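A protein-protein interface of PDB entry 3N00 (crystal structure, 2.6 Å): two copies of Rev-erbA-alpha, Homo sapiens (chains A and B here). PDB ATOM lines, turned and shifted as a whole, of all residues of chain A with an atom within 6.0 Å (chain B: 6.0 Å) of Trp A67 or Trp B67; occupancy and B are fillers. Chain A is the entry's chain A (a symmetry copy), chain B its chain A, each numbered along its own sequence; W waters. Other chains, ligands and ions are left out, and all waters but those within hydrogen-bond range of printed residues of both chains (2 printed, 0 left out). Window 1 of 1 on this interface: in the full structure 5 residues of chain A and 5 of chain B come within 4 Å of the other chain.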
ATOM      1  N   VAL A  63      18.145 -10.054 -30.865  1.00  0.00           N
ATOM      2  CA  VAL A  63      17.066 -10.661 -30.082  1.00  0.00           C
ATOM      3  C   VAL A  63      16.483  -9.547 -29.188  1.00  0.00           C
ATOM      4  O   VAL A  63      15.408  -8.992 -29.476  1.00  0.00           O
ATOM      5  CB  VAL A  63      17.581 -11.902 -29.274  1.00  0.00           C
ATOM      6  CG1 VAL A  63      16.520 -13.004 -29.250  1.00  0.00           C
ATOM      7  CG2 VAL A  63      18.903 -12.418 -29.866  1.00  0.00           C
ATOM      8  N   GLN A  64      17.181  -9.259 -28.093  1.00  0.00           N
ATOM      9  CA  GLN A  64      17.214  -7.934 -27.488  1.00  0.00           C
ATOM     10  C   GLN A  64      18.656  -7.450 -27.519  1.00  0.00           C
ATOM     11  O   GLN A  64      18.956  -6.327 -27.095  1.00  0.00           O
ATOM     12  CB  GLN A  64      16.746  -7.976 -26.036  1.00  0.00           C
ATOM     13  CG  GLN A  64      17.782  -8.527 -25.035  1.00  0.00           C
ATOM     14  CD  GLN A  64      17.660  -7.909 -23.648  1.00  0.00           C
ATOM     15  OE1 GLN A  64      16.961  -6.906 -23.460  1.00  0.00           O
ATOM     16  NE2 GLN A  64      18.349  -8.499 -22.668  1.00  0.00           N
ATOM     17  N   GLU A  65      19.553  -8.330 -27.964  1.00  0.00           N
ATOM     18  CA  GLU A  65      20.938  -7.985 -28.159  1.00  0.00           C
ATOM     19  C   GLU A  65      21.006  -6.980 -29.303  1.00  0.00           C
ATOM     20  O   GLU A  65      21.850  -6.090 -29.283  1.00  0.00           O
ATOM     21  CB  GLU A  65      21.771  -9.240 -28.462  1.00  0.00           C
ATOM     22  N   ILE A  66      20.106  -7.101 -30.278  1.00  0.00           N
ATOM     23  CA  ILE A  66      20.036  -6.136 -31.386  1.00  0.00           C
ATOM     24  C   ILE A  66      19.633  -4.725 -30.905  1.00  0.00           C
ATOM     25  O   ILE A  66      20.142  -3.708 -31.406  1.00  0.00           O
ATOM     26  CB  ILE A  66      19.040  -6.584 -32.493  1.00  0.00           C
ATOM     27  CG1 ILE A  66      19.465  -7.921 -33.115  1.00  0.00           C
ATOM     28  N   TRP A  67      18.721  -4.676 -29.934  1.00  0.00           N
ATOM     29  CA  TRP A  67      18.222  -3.417 -29.383  1.00  0.00           C
ATOM     30  C   TRP A  67      19.280  -2.718 -28.531  1.00  0.00           C
ATOM     31  O   TRP A  67      19.478  -1.505 -28.638  1.00  0.00           O
ATOM     32  CB  TRP A  67      16.953  -3.664 -28.557  1.00  0.00           C
ATOM     33  CG  TRP A  67      16.251  -2.419 -28.134  1.00  0.00           C
ATOM     34  CD1 TRP A  67      16.358  -1.190 -28.702  1.00  0.00           C
ATOM     35  CD2 TRP A  67      15.295  -2.291 -27.082  1.00  0.00           C
ATOM     36  NE1 TRP A  67      15.550  -0.298 -28.059  1.00  0.00           N
ATOM     37  CE2 TRP A  67      14.883  -0.942 -27.058  1.00  0.00           C
ATOM     38  CE3 TRP A  67      14.754  -3.177 -26.149  1.00  0.00           C
ATOM     39  CZ2 TRP A  67      13.961  -0.451 -26.130  1.00  0.00           C
ATOM     40  CZ3 TRP A  67      13.829  -2.689 -25.227  1.00  0.00           C
ATOM     41  CH2 TRP A  67      13.447  -1.335 -25.227  1.00  0.00           C
ATOM     42  N   GLU A  68      19.950  -3.491 -27.684  1.00  0.00           N
ATOM     43  CA  GLU A  68      21.085  -2.986 -26.927  1.00  0.00           C
ATOM     44  C   GLU A  68      22.180  -2.460 -27.868  1.00  0.00           C
ATOM     45  O   GLU A  68      22.793  -1.435 -27.578  1.00  0.00           O
ATOM     46  CB  GLU A  68      21.639  -4.075 -25.992  1.00  0.00           C
ATOM     47  CG  GLU A  68      20.696  -4.473 -24.820  1.00  0.00           C
ATOM     48  CD  GLU A  68      21.239  -5.618 -23.931  1.00  0.00           C
ATOM     49  OE1 GLU A  68      22.166  -6.360 -24.354  1.00  0.00           O
ATOM     50  OE2 GLU A  68      20.724  -5.771 -22.794  1.00  0.00           O
ATOM     51  N   ASP A  69      22.399  -3.145 -28.996  1.00  0.00           N
ATOM     52  CA  ASP A  69      23.489  -2.819 -29.939  1.00  0.00           C
ATOM     53  C   ASP A  69      23.218  -1.526 -30.707  1.00  0.00           C
ATOM     54  O   ASP A  69      24.094  -0.659 -30.838  1.00  0.00           O
ATOM     55  N   PHE A  70      21.995  -1.422 -31.217  1.00  0.00           N
ATOM     56  CA  PHE A  70      21.463  -0.175 -31.742  1.00  0.00           C
ATOM     57  C   PHE A  70      21.521   0.948 -30.693  1.00  0.00           C
ATOM     58  O   PHE A  70      21.956   2.062 -30.987  1.00  0.00           O
ATOM     59  CB  PHE A  70      20.017  -0.410 -32.164  1.00  0.00           C
ATOM     60  CG  PHE A  70      19.348   0.789 -32.761  1.00  0.00           C
ATOM     61  CD1 PHE A  70      19.766   1.292 -33.985  1.00  0.00           C
ATOM     62  CD2 PHE A  70      18.273   1.399 -32.118  1.00  0.00           C
ATOM     63  CE1 PHE A  70      19.134   2.401 -34.560  1.00  0.00           C
ATOM     64  CE2 PHE A  70      17.631   2.508 -32.682  1.00  0.00           C
ATOM     65  CZ  PHE A  70      18.063   3.008 -33.904  1.00  0.00           C
ATOM     66  N   SER A  71      21.110   0.643 -29.465  1.00  0.00           N
ATOM     67  CA  SER A  71      21.019   1.661 -28.424  1.00  0.00           C
ATOM     68  C   SER A  71      22.361   2.328 -28.160  1.00  0.00           C
ATOM     69  O   SER A  71      22.425   3.543 -28.020  1.00  0.00           O
ATOM     70  CB  SER A  71      20.451   1.078 -27.139  1.00  0.00           C
ATOM     71  OG  SER A  71      19.109   0.689 -27.336  1.00  0.00           O
ATOM     72  N   MET A  72      23.431   1.547 -28.119  1.00  0.00           N
ATOM     73  CA  MET A  72      24.771   2.094 -27.844  1.00  0.00           C
ATOM     74  C   MET A  72      25.510   2.642 -29.060  1.00  0.00           C
ATOM     75  O   MET A  72      26.604   3.189 -28.924  1.00  0.00           O
ATOM     76  CB  MET A  72      25.648   1.022 -27.225  1.00  0.00           C
ATOM     77  CG  MET A  72      25.515   0.892 -25.731  1.00  0.00           C
ATOM     78  SD  MET A  72      26.701  -0.359 -25.244  1.00  0.00           S
ATOM     79  CE  MET A  72      26.144  -1.769 -26.240  1.00  0.00           C
ATOM     80  N   MET A 142      12.133  -4.729 -32.580  1.00  0.00           N
ATOM     81  CA  MET A 142      12.570  -3.961 -31.404  1.00  0.00           C
ATOM     82  C   MET A 142      11.743  -2.674 -31.180  1.00  0.00           C
ATOM     83  O   MET A 142      11.831  -2.057 -30.109  1.00  0.00           O
ATOM     84  CB  MET A 142      14.076  -3.640 -31.495  1.00  0.00           C
ATOM     85  CG  MET A 142      14.465  -2.646 -32.593  1.00  0.00           C
ATOM     86  SD  MET A 142      16.208  -2.209 -32.621  1.00  0.00           S
ATOM     87  CE  MET A 142      16.965  -3.833 -32.594  1.00  0.00           C
ATOM     88  N   LEU A 237      12.245   4.414 -27.797  1.00  0.00           N
ATOM     89  CA  LEU A 237      12.955   3.953 -26.602  1.00  0.00           C
ATOM     90  C   LEU A 237      14.272   3.313 -26.958  1.00  0.00           C
ATOM     91  O   LEU A 237      14.336   2.499 -27.860  1.00  0.00           O
ATOM     92  CB  LEU A 237      12.131   2.929 -25.818  1.00  0.00           C
ATOM     93  CG  LEU A 237      10.972   3.447 -24.966  1.00  0.00           C
ATOM     94  CD1 LEU A 237      10.318   2.251 -24.296  1.00  0.00           C
ATOM     95  CD2 LEU A 237      11.407   4.487 -23.938  1.00  0.00           C
ATOM     96  N   LEU A 238      15.314   3.697 -26.240  1.00  0.00           N
ATOM     97  CA  LEU A 238      16.550   2.955 -26.225  1.00  0.00           C
ATOM     98  C   LEU A 238      16.592   2.097 -24.968  1.00  0.00           C
ATOM     99  O   LEU A 238      15.775   2.249 -24.067  1.00  0.00           O
ATOM    100  CB  LEU A 238      17.735   3.918 -26.258  1.00  0.00           C
ATOM    101  CG  LEU A 238      17.833   4.781 -27.519  1.00  0.00           C
ATOM    102  CD1 LEU A 238      19.223   5.385 -27.600  1.00  0.00           C
ATOM    103  CD2 LEU A 238      17.519   3.979 -28.788  1.00  0.00           C
ATOM    104  N   SER A 239      17.552   1.190 -24.917  1.00  0.00           N
ATOM    105  CA  SER A 239      17.668   0.257 -23.808  1.00  0.00           C
ATOM    106  C   SER A 239      19.121   0.035 -23.445  1.00  0.00           C
ATOM    107  O   SER A 239      19.939  -0.256 -24.320  1.00  0.00           O
ATOM    108  CB  SER A 239      17.049  -1.075 -24.200  1.00  0.00           C
ATOM    109  OG  SER A 239      16.961  -1.928 -23.083  1.00  0.00           O
ATOM    110  N   VAL B  63       3.050   4.707 -24.775  1.00  0.00           N
ATOM    111  CA  VAL B  63       4.338   5.332 -25.084  1.00  0.00           C
ATOM    112  C   VAL B  63       5.423   4.262 -24.842  1.00  0.00           C
ATOM    113  O   VAL B  63       5.951   3.659 -25.792  1.00  0.00           O
ATOM    114  CB  VAL B  63       4.552   6.637 -24.240  1.00  0.00           C
ATOM    115  CG1 VAL B  63       5.254   7.707 -25.078  1.00  0.00           C
ATOM    116  CG2 VAL B  63       3.209   7.151 -23.696  1.00  0.00           C
ATOM    117  N   GLN B  64       5.768   4.065 -23.571  1.00  0.00           N
ATOM    118  CA  GLN B  64       6.230   2.783 -23.055  1.00  0.00           C
ATOM    119  C   GLN B  64       5.248   2.339 -21.981  1.00  0.00           C
ATOM    120  O   GLN B  64       5.389   1.255 -21.403  1.00  0.00           O
ATOM    121  CB  GLN B  64       7.615   2.906 -22.427  1.00  0.00           C
ATOM    122  CG  GLN B  64       7.639   3.549 -21.026  1.00  0.00           C
ATOM    123  CD  GLN B  64       8.762   3.018 -20.143  1.00  0.00           C
ATOM    124  OE1 GLN B  64       9.401   2.010 -20.468  1.00  0.00           O
ATOM    125  NE2 GLN B  64       9.003   3.690 -19.014  1.00  0.00           N
ATOM    126  N   GLU B  65       4.290   3.214 -21.676  1.00  0.00           N
ATOM    127  CA  GLU B  65       3.220   2.897 -20.763  1.00  0.00           C
ATOM    128  C   GLU B  65       2.360   1.822 -21.417  1.00  0.00           C
ATOM    129  O   GLU B  65       1.831   0.960 -20.724  1.00  0.00           O
ATOM    130  CB  GLU B  65       2.400   4.153 -20.433  1.00  0.00           C
ATOM    131  N   ILE B  66       2.244   1.855 -22.744  1.00  0.00           N
ATOM    132  CA  ILE B  66       1.502   0.819 -23.478  1.00  0.00           C
ATOM    133  C   ILE B  66       2.169  -0.569 -23.361  1.00  0.00           C
ATOM    134  O   ILE B  66       1.484  -1.601 -23.257  1.00  0.00           O
ATOM    135  CB  ILE B  66       1.344   1.166 -24.986  1.00  0.00           C
ATOM    136  CG1 ILE B  66       0.561   2.472 -25.176  1.00  0.00           C
ATOM    137  N   TRP B  67       3.502  -0.581 -23.378  1.00  0.00           N
ATOM    138  CA  TRP B  67       4.280  -1.816 -23.295  1.00  0.00           C
ATOM    139  C   TRP B  67       4.215  -2.429 -21.897  1.00  0.00           C
ATOM    140  O   TRP B  67       4.037  -3.640 -21.744  1.00  0.00           O
ATOM    141  CB  TRP B  67       5.738  -1.552 -23.692  1.00  0.00           C
ATOM    142  CG  TRP B  67       6.560  -2.787 -23.845  1.00  0.00           C
ATOM    143  CD1 TRP B  67       6.104  -4.047 -24.068  1.00  0.00           C
ATOM    144  CD2 TRP B  67       7.984  -2.875 -23.834  1.00  0.00           C
ATOM    145  NE1 TRP B  67       7.147  -4.918 -24.175  1.00  0.00           N
ATOM    146  CE2 TRP B  67       8.318  -4.230 -24.035  1.00  0.00           C
ATOM    147  CE3 TRP B  67       9.012  -1.945 -23.664  1.00  0.00           C
ATOM    148  CZ2 TRP B  67       9.638  -4.686 -24.060  1.00  0.00           C
ATOM    149  CZ3 TRP B  67      10.330  -2.400 -23.695  1.00  0.00           C
ATOM    150  CH2 TRP B  67      10.626  -3.761 -23.889  1.00  0.00           C
ATOM    151  N   GLU B  68       4.365  -1.584 -20.882  1.00  0.00           N
ATOM    152  CA  GLU B  68       4.172  -2.007 -19.504  1.00  0.00           C
ATOM    153  C   GLU B  68       2.754  -2.561 -19.295  1.00  0.00           C
ATOM    154  O   GLU B  68       2.584  -3.547 -18.583  1.00  0.00           O
ATOM    155  CB  GLU B  68       4.457  -0.845 -18.537  1.00  0.00           C
ATOM    156  CG  GLU B  68       5.946  -0.398 -18.471  1.00  0.00           C
ATOM    157  CD  GLU B  68       6.204   0.816 -17.547  1.00  0.00           C
ATOM    158  OE1 GLU B  68       5.245   1.556 -17.195  1.00  0.00           O
ATOM    159  OE2 GLU B  68       7.385   1.028 -17.171  1.00  0.00           O
ATOM    160  N   ASP B  69       1.755  -1.944 -19.936  1.00  0.00           N
ATOM    161  CA  ASP B  69       0.333  -2.299 -19.745  1.00  0.00           C
ATOM    162  C   ASP B  69      -0.013  -3.646 -20.377  1.00  0.00           C
ATOM    163  O   ASP B  69      -0.676  -4.494 -19.765  1.00  0.00           O
ATOM    164  N   PHE B  70       0.439  -3.817 -21.616  1.00  0.00           N
ATOM    165  CA  PHE B  70       0.446  -5.110 -22.281  1.00  0.00           C
ATOM    166  C   PHE B  70       1.212  -6.161 -21.461  1.00  0.00           C
ATOM    167  O   PHE B  70       0.734  -7.279 -21.266  1.00  0.00           O
ATOM    168  CB  PHE B  70       1.103  -4.944 -23.646  1.00  0.00           C
ATOM    169  CG  PHE B  70       1.148  -6.197 -24.464  1.00  0.00           C
ATOM    170  CD1 PHE B  70      -0.023  -6.766 -24.946  1.00  0.00           C
ATOM    171  CD2 PHE B  70       2.365  -6.794 -24.785  1.00  0.00           C
ATOM    172  CE1 PHE B  70       0.012  -7.927 -25.727  1.00  0.00           C
ATOM    173  CE2 PHE B  70       2.414  -7.955 -25.567  1.00  0.00           C
ATOM    174  CZ  PHE B  70       1.235  -8.521 -26.037  1.00  0.00           C
ATOM    175  N   SER B  71       2.386  -5.790 -20.958  1.00  0.00           N
ATOM    176  CA  SER B  71       3.244  -6.741 -20.260  1.00  0.00           C
ATOM    177  C   SER B  71       2.553  -7.351 -19.050  1.00  0.00           C
ATOM    178  O   SER B  71       2.647  -8.551 -18.830  1.00  0.00           O
ATOM    179  CB  SER B  71       4.559  -6.092 -19.852  1.00  0.00           C
ATOM    180  OG  SER B  71       5.308  -5.755 -21.001  1.00  0.00           O
ATOM    181  N   MET B  72       1.839  -6.539 -18.283  1.00  0.00           N
ATOM    182  CA  MET B  72       1.154  -7.028 -17.075  1.00  0.00           C
ATOM    183  C   MET B  72      -0.227  -7.632 -17.311  1.00  0.00           C
ATOM    184  O   MET B  72      -0.849  -8.138 -16.379  1.00  0.00           O
ATOM    185  CB  MET B  72       0.988  -5.894 -16.081  1.00  0.00           C
ATOM    186  CG  MET B  72       2.176  -5.672 -15.183  1.00  0.00           C
ATOM    187  SD  MET B  72       1.699  -4.359 -14.061  1.00  0.00           S
ATOM    188  CE  MET B  72       1.301  -3.032 -15.232  1.00  0.00           C
ATOM    189  N   MET B 142       5.993  -0.886 -30.020  1.00  0.00           N
ATOM    190  CA  MET B 142       6.587  -1.564 -28.857  1.00  0.00           C
ATOM    191  C   MET B 142       7.347  -2.857 -29.234  1.00  0.00           C
ATOM    192  O   MET B 142       8.095  -3.401 -28.409  1.00  0.00           O
ATOM    193  CB  MET B 142       5.512  -1.848 -27.787  1.00  0.00           C
ATOM    194  CG  MET B 142       4.469  -2.899 -28.174  1.00  0.00           C
ATOM    195  SD  MET B 142       3.285  -3.287 -26.879  1.00  0.00           S
ATOM    196  CE  MET B 142       2.748  -1.643 -26.407  1.00  0.00           C
ATOM    197  N   LEU B 237       9.705  -9.696 -26.133  1.00  0.00           N
ATOM    198  CA  LEU B 237      10.094  -9.138 -24.835  1.00  0.00           C
ATOM    199  C   LEU B 237       8.925  -8.485 -24.146  1.00  0.00           C
ATOM    200  O   LEU B 237       8.193  -7.730 -24.756  1.00  0.00           O
ATOM    201  CB  LEU B 237      11.199  -8.090 -24.982  1.00  0.00           C
ATOM    202  CG  LEU B 237      12.624  -8.584 -25.231  1.00  0.00           C
ATOM    203  CD1 LEU B 237      13.526  -7.367 -25.340  1.00  0.00           C
ATOM    204  CD2 LEU B 237      13.119  -9.544 -24.152  1.00  0.00           C
ATOM    205  N   LEU B 238       8.762  -8.792 -22.869  1.00  0.00           N
ATOM    206  CA  LEU B 238       7.918  -8.016 -21.995  1.00  0.00           C
ATOM    207  C   LEU B 238       8.793  -7.078 -21.175  1.00  0.00           C
ATOM    208  O   LEU B 238      10.013  -7.196 -21.161  1.00  0.00           O
ATOM    209  CB  LEU B 238       7.122  -8.946 -21.081  1.00  0.00           C
ATOM    210  CG  LEU B 238       6.150  -9.885 -21.802  1.00  0.00           C
ATOM    211  CD1 LEU B 238       5.170 -10.453 -20.791  1.00  0.00           C
ATOM    212  CD2 LEU B 238       5.403  -9.175 -22.936  1.00  0.00           C
ATOM    213  N   SER B 239       8.157  -6.143 -20.491  1.00  0.00           N
ATOM    214  CA  SER B 239       8.870  -5.137 -19.719  1.00  0.00           C
ATOM    215  C   SER B 239       8.151  -4.851 -18.418  1.00  0.00           C
ATOM    216  O   SER B 239       6.946  -4.594 -18.421  1.00  0.00           O
ATOM    217  CB  SER B 239       8.961  -3.851 -20.526  1.00  0.00           C
ATOM    218  OG  SER B 239       9.820  -2.932 -19.894  1.00  0.00           O
HETATM  219  O   HOH W   1      11.535  -3.524 -28.124  1.00  0.00           O
HETATM  220  O   HOH W   2       9.717  -1.818 -27.387  1.00  0.00           O
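The backbone carbonyl oxygen (O) of Trp B67 lies within hydrogen-bond range of the side-chain hydroxyl (OG) of Ser B71, 2.6 Å away.
The indole nitrogen (NE1) of Trp B67 lies within hydrogen-bond range of the backbone carbonyl oxygen (O) of Leu B237, 3.1 Å away.
O of Trp A67 sits at hydrogen-bond distance from OG of Ser A71 (2.6 Å).
The backbone carbonyl oxygen (O) of Leu A237 sits at hydrogen-bond distance from the indole nitrogen (NE1) of Trp A67, at 3.1 Å.
CD1 of Leu B237 touches CB of Gln A64 (3.4 Å).
Trp B67 touches Trp A67 (CZ3 to CH2, 3.6 Å).
Leu A237 touches Gln B64 (CD1 to CB, 3.4 Å).
Of the printed residues of chain B, Gln A64 touches Leu B237 (3.4 Å).
Ile A66 touches none of the printed residues of chain B.
Of chain B, only Trp B67 (3.6 Å) comes within 4 Å of Trp A67.
Phe A70 touches none of the printed residues of chain B.
Printed residues of chain A within 4 Å of Gln B64: Leu A237 (3.4 Å).
Trp B67 touches one residue of chain A.
The nearest residue of chain A that does not touch Trp B67 is Leu A237 (4.4 Å).
The nearest printed residue of chain B that does not touch Leu A237 is Trp B67 (4.4 Å).
Hydrophobic or aromatic side chains of chain A within 4 Å of the printed part of chain B: Trp A67 and Leu A237.
Of the 14 printed residues of chain B, 3 touch a printed residue of chain A.
Hydrophobic or aromatic side chains of chain B within 4 Å of the printed part of chain A: Trp B67 and Leu B237.
Gln A64 touches Leu B237, and with the chains exchanged Leu A237 touches Gln B64.
Trp A67 touches its own counterpart, Trp B67.
Of the 3 pairs that touch across the chains among the printed residues, 3 have their exchanged pair printed and touching as well.
Water W2 bridges the backbone carbonyl oxygen (O) of Met B142 (2.5 Å) and the backbone carbonyl oxygen (O) of Met A142 (3.5 Å).
Water W1 lies within hydrogen-bond range of the backbone carbonyl oxygen of Met A142 (2.5 Å) and the backbone carbonyl oxygen of Met B142 (3.5 Å).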
